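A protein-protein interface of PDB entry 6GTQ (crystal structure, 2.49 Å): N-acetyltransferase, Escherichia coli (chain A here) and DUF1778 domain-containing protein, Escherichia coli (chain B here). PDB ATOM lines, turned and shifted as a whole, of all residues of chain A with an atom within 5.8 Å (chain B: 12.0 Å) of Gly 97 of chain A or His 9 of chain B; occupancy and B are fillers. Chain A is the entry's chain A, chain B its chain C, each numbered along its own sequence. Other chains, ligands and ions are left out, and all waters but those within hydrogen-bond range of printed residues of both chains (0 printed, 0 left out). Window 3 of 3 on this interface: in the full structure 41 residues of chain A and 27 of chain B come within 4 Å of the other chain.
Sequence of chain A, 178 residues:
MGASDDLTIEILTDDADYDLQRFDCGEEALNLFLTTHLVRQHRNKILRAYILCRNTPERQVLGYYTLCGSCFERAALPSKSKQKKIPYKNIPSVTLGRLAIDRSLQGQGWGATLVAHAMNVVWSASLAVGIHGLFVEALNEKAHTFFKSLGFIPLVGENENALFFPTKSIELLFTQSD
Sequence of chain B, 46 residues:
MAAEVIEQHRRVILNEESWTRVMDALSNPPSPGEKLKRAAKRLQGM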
ATOM      1  N   THR A  66     -27.153  25.570  28.782  1.00  0.00           N
ATOM      2  CA  THR A  66     -27.464  24.540  27.779  1.00  0.00           C
ATOM      3  C   THR A  66     -27.025  23.164  28.271  1.00  0.00           C
ATOM      4  O   THR A  66     -25.967  23.042  28.883  1.00  0.00           O
ATOM      5  CB  THR A  66     -26.911  24.868  26.369  1.00  0.00           C
ATOM      6  OG1 THR A  66     -25.482  24.810  26.374  1.00  0.00           O
ATOM      7  CG2 THR A  66     -27.398  26.204  25.828  1.00  0.00           C
ATOM      8  N   LEU A  67     -27.853  22.139  28.006  1.00  0.00           N
ATOM      9  CA  LEU A  67     -27.603  20.739  28.342  1.00  0.00           C
ATOM     10  C   LEU A  67     -27.722  19.856  27.121  1.00  0.00           C
ATOM     11  O   LEU A  67     -28.548  20.108  26.227  1.00  0.00           O
ATOM     12  CB  LEU A  67     -28.646  20.210  29.342  1.00  0.00           C
ATOM     13  CG  LEU A  67     -28.623  20.664  30.778  1.00  0.00           C
ATOM     14  CD1 LEU A  67     -29.793  20.064  31.513  1.00  0.00           C
ATOM     15  CD2 LEU A  67     -27.320  20.278  31.481  1.00  0.00           C
ATOM     16  N   THR A  95     -23.836  16.831  29.573  1.00  0.00           N
ATOM     17  CA  THR A  95     -22.884  17.936  29.552  1.00  0.00           C
ATOM     18  C   THR A  95     -23.610  19.280  29.642  1.00  0.00           C
ATOM     19  O   THR A  95     -24.559  19.520  28.895  1.00  0.00           O
ATOM     20  CB  THR A  95     -21.970  17.847  28.322  1.00  0.00           C
ATOM     21  OG1 THR A  95     -21.286  16.601  28.340  1.00  0.00           O
ATOM     22  CG2 THR A  95     -20.954  18.966  28.265  1.00  0.00           C
ATOM     23  N   LEU A  96     -23.147  20.152  30.552  1.00  0.00           N
ATOM     24  CA  LEU A  96     -23.597  21.535  30.664  1.00  0.00           C
ATOM     25  C   LEU A  96     -22.496  22.279  29.886  1.00  0.00           C
ATOM     26  O   LEU A  96     -21.380  22.433  30.392  1.00  0.00           O
ATOM     27  CB  LEU A  96     -23.628  21.983  32.132  1.00  0.00           C
ATOM     28  CG  LEU A  96     -24.594  23.119  32.530  1.00  0.00           C
ATOM     29  CD1 LEU A  96     -24.586  23.314  34.033  1.00  0.00           C
ATOM     30  CD2 LEU A  96     -24.212  24.427  31.912  1.00  0.00           C
ATOM     31  N   GLY A  97     -22.790  22.633  28.635  1.00  0.00           N
ATOM     32  CA  GLY A  97     -21.824  23.249  27.729  1.00  0.00           C
ATOM     33  C   GLY A  97     -21.706  24.757  27.731  1.00  0.00           C
ATOM     34  O   GLY A  97     -20.707  25.290  27.245  1.00  0.00           O
ATOM     35  N   ARG A  98     -22.722  25.454  28.235  1.00  0.00           N
ATOM     36  CA  ARG A  98     -22.755  26.913  28.273  1.00  0.00           C
ATOM     37  C   ARG A  98     -23.500  27.388  29.485  1.00  0.00           C
ATOM     38  O   ARG A  98     -24.550  26.848  29.820  1.00  0.00           O
ATOM     39  CB  ARG A  98     -23.428  27.486  27.006  1.00  0.00           C
ATOM     40  CG  ARG A  98     -22.468  27.743  25.867  1.00  0.00           C
ATOM     41  CD  ARG A  98     -23.146  27.644  24.534  1.00  0.00           C
ATOM     42  NE  ARG A  98     -22.240  27.987  23.439  1.00  0.00           N
ATOM     43  CZ  ARG A  98     -22.034  27.238  22.359  1.00  0.00           C
ATOM     44  NH1 ARG A  98     -21.187  27.639  21.418  1.00  0.00           N
ATOM     45  NH2 ARG A  98     -22.684  26.091  22.203  1.00  0.00           N
ATOM     46  N   LEU A  99     -22.965  28.423  30.126  1.00  0.00           N
ATOM     47  CA  LEU A  99     -23.549  29.083  31.286  1.00  0.00           C
ATOM     48  C   LEU A  99     -23.198  30.553  31.188  1.00  0.00           C
ATOM     49  O   LEU A  99     -22.019  30.905  31.084  1.00  0.00           O
ATOM     50  CB  LEU A  99     -23.052  28.456  32.616  1.00  0.00           C
ATOM     51  CG  LEU A  99     -23.607  29.044  33.932  1.00  0.00           C
ATOM     52  CD1 LEU A  99     -25.037  28.610  34.193  1.00  0.00           C
ATOM     53  CD2 LEU A  99     -22.755  28.632  35.104  1.00  0.00           C
ATOM     54  N   PHE A 135     -20.995  16.634  33.465  1.00  0.00           N
ATOM     55  CA  PHE A 135     -19.742  17.219  32.994  1.00  0.00           C
ATOM     56  C   PHE A 135     -20.011  18.666  32.665  1.00  0.00           C
ATOM     57  O   PHE A 135     -21.117  19.013  32.268  1.00  0.00           O
ATOM     58  CB  PHE A 135     -19.196  16.486  31.763  1.00  0.00           C
ATOM     59  CG  PHE A 135     -18.602  15.139  32.082  1.00  0.00           C
ATOM     60  CD1 PHE A 135     -19.389  13.995  32.073  1.00  0.00           C
ATOM     61  CD2 PHE A 135     -17.256  15.014  32.413  1.00  0.00           C
ATOM     62  CE1 PHE A 135     -18.832  12.744  32.371  1.00  0.00           C
ATOM     63  CE2 PHE A 135     -16.707  13.769  32.717  1.00  0.00           C
ATOM     64  CZ  PHE A 135     -17.497  12.643  32.689  1.00  0.00           C
ATOM     65  N   VAL A 136     -19.011  19.518  32.847  1.00  0.00           N
ATOM     66  CA  VAL A 136     -19.162  20.941  32.585  1.00  0.00           C
ATOM     67  C   VAL A 136     -17.960  21.474  31.805  1.00  0.00           C
ATOM     68  O   VAL A 136     -16.859  20.943  31.934  1.00  0.00           O
ATOM     69  CB  VAL A 136     -19.487  21.714  33.892  1.00  0.00           C
ATOM     70  CG1 VAL A 136     -18.240  22.079  34.686  1.00  0.00           C
ATOM     71  CG2 VAL A 136     -20.326  22.936  33.603  1.00  0.00           C
ATOM     72  N   GLU A 137     -18.195  22.476  30.950  1.00  0.00           N
ATOM     73  CA  GLU A 137     -17.158  23.095  30.120  1.00  0.00           C
ATOM     74  C   GLU A 137     -16.710  24.441  30.703  1.00  0.00           C
ATOM     75  O   GLU A 137     -17.529  25.357  30.838  1.00  0.00           O
ATOM     76  CB  GLU A 137     -17.644  23.256  28.658  1.00  0.00           C
ATOM     77  CG  GLU A 137     -17.865  21.947  27.906  1.00  0.00           C
ATOM     78  CD  GLU A 137     -16.649  21.049  27.723  1.00  0.00           C
ATOM     79  OE1 GLU A 137     -15.579  21.557  27.312  1.00  0.00           O
ATOM     80  OE2 GLU A 137     -16.772  19.830  27.985  1.00  0.00           O
ATOM     81  N   HIS B   9     -20.048  21.880  25.062  1.00  0.00           N
ATOM     82  CA  HIS B   9     -20.548  21.406  23.771  1.00  0.00           C
ATOM     83  C   HIS B   9     -20.020  19.994  23.416  1.00  0.00           C
ATOM     84  O   HIS B   9     -20.140  19.555  22.264  1.00  0.00           O
ATOM     85  CB  HIS B   9     -20.170  22.393  22.665  1.00  0.00           C
ATOM     86  N   ARG B  10     -19.470  19.278  24.422  1.00  0.00           N
ATOM     87  CA  ARG B  10     -18.870  17.948  24.262  1.00  0.00           C
ATOM     88  C   ARG B  10     -19.825  16.775  24.566  1.00  0.00           C
ATOM     89  O   ARG B  10     -20.263  16.593  25.707  1.00  0.00           O
ATOM     90  CB  ARG B  10     -17.577  17.840  25.096  1.00  0.00           C
ATOM     91  CG  ARG B  10     -16.607  16.766  24.619  1.00  0.00           C
ATOM     92  CD  ARG B  10     -15.313  16.825  25.400  1.00  0.00           C
ATOM     93  NE  ARG B  10     -14.385  15.761  25.016  1.00  0.00           N
ATOM     94  CZ  ARG B  10     -13.411  15.893  24.120  1.00  0.00           C
ATOM     95  NH1 ARG B  10     -13.222  17.051  23.499  1.00  0.00           N
ATOM     96  NH2 ARG B  10     -12.619  14.867  23.836  1.00  0.00           N
ATOM     97  N   ARG B  11     -20.110  15.967  23.526  1.00  0.00           N
ATOM     98  CA  ARG B  11     -20.940  14.757  23.587  1.00  0.00           C
ATOM     99  C   ARG B  11     -20.047  13.492  23.644  1.00  0.00           C
ATOM    100  O   ARG B  11     -20.535  12.414  23.992  1.00  0.00           O
ATOM    101  CB  ARG B  11     -21.906  14.683  22.384  1.00  0.00           C
ATOM    102  N   VAL B  12     -18.768  13.647  23.331  1.00  0.00           N
ATOM    103  CA  VAL B  12     -17.787  12.580  23.399  1.00  0.00           C
ATOM    104  C   VAL B  12     -16.626  13.023  24.275  1.00  0.00           C
ATOM    105  O   VAL B  12     -15.678  13.661  23.854  1.00  0.00           O
ATOM    106  CB  VAL B  12     -17.225  12.196  22.023  1.00  0.00           C
ATOM    107  CG1 VAL B  12     -16.475  13.350  21.383  1.00  0.00           C
ATOM    108  CG2 VAL B  12     -16.371  10.954  22.130  1.00  0.00           C
ATOM    109  N   ILE B  13     -16.694  12.619  25.519  1.00  0.00           N
ATOM    110  CA  ILE B  13     -15.662  12.932  26.468  1.00  0.00           C
ATOM    111  C   ILE B  13     -14.615  11.797  26.411  1.00  0.00           C
ATOM    112  O   ILE B  13     -14.892  10.697  26.814  1.00  0.00           O
ATOM    113  CB  ILE B  13     -16.316  13.069  27.862  1.00  0.00           C
ATOM    114  CG1 ILE B  13     -17.368  14.146  27.853  1.00  0.00           C
ATOM    115  CG2 ILE B  13     -15.341  13.516  28.903  1.00  0.00           C
ATOM    116  CD1 ILE B  13     -18.541  13.823  28.720  1.00  0.00           C
ATOM    117  N   LEU B  14     -13.415  12.086  25.920  1.00  0.00           N
ATOM    118  CA  LEU B  14     -12.316  11.106  25.814  1.00  0.00           C
ATOM    119  C   LEU B  14     -11.248  11.310  26.910  1.00  0.00           C
ATOM    120  O   LEU B  14     -10.373  12.159  26.748  1.00  0.00           O
ATOM    121  CB  LEU B  14     -11.694  11.154  24.406  1.00  0.00           C
ATOM    122  CG  LEU B  14     -12.625  10.735  23.277  1.00  0.00           C
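OG1 of Thr 95 of chain A is in hydrogen-bond range of O of Arg 10 of chain B, at 2.8 Å.
Of chain B, only His 9 (3.5 Å) comes within 4 Å of Gly 97 of chain A.
His 9 of chain B touches two residues of chain A.
Of chain B, only Arg 10 (2.8 Å) and Ile 13 (3.9 Å) come within 4 Å of Thr 95 of chain A.
No residue of chain B comes within 4 Å of Arg 98 of chain A.
Val 136 of chain A touches none of the printed residues of chain B.
Printed residues of chain B within 4 Å of Phe 135 of chain A: Ile 13.
Printed residues of chain A within 4 Å of Arg 10 of chain B: Thr 95 (2.8 Å) and Glu 137 (3.6 Å).
Printed residues of chain A within 4 Å of Ile 13 of chain B: Thr 95 (3.9 Å) and Phe 135 (3.5 Å).
Val 12 of chain B touches none of the printed residues of chain A.
The nearest residue of chain B that does not touch Gly 97 of chain A is Arg 10 of chain B (5.7 Å).
The backbone carbonyl oxygen (O) of Thr 66 of chain A lies within hydrogen-bond range of the backbone NH (N) of Gly 97 of chain A (3.2 Å).
O of Phe 135 of chain A sits at hydrogen-bond distance from N of Leu 96 of chain A (2.9 Å).
The backbone carbonyl oxygen (O) of Leu 96 of chain A sits at hydrogen-bond distance from the backbone NH (N) of Glu 137 of chain A, at 3.2 Å.
The guanidinium group (NE) of Arg 10 of chain B is in hydrogen-bond range of the backbone carbonyl oxygen (O) of Val 12 of chain B (2.7 Å).
Among the printed residues, pairs that only touch across the chains: Thr 95 of chain A with Ile 13 of chain B (3.9 Å), Gly 97 of chain A with His 9 of chain B (3.5 Å), Phe 135 of chain A with Ile 13 of chain B (3.5 Å), Glu 137 of chain A with His 9 of chain B (3.6 Å) and Glu 137 of chain A with Arg 10 of chain B (3.6 Å).
Printed residues of chain B that touch a printed residue of chain A: His 9, Arg 10 and Ile 13.
Among the printed residues, 6 pairs touch across the chains.
Among the printed residues, no Asp or Glu carboxylate lies within 4 Å of a Lys or Arg side-chain nitrogen of the other chain.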
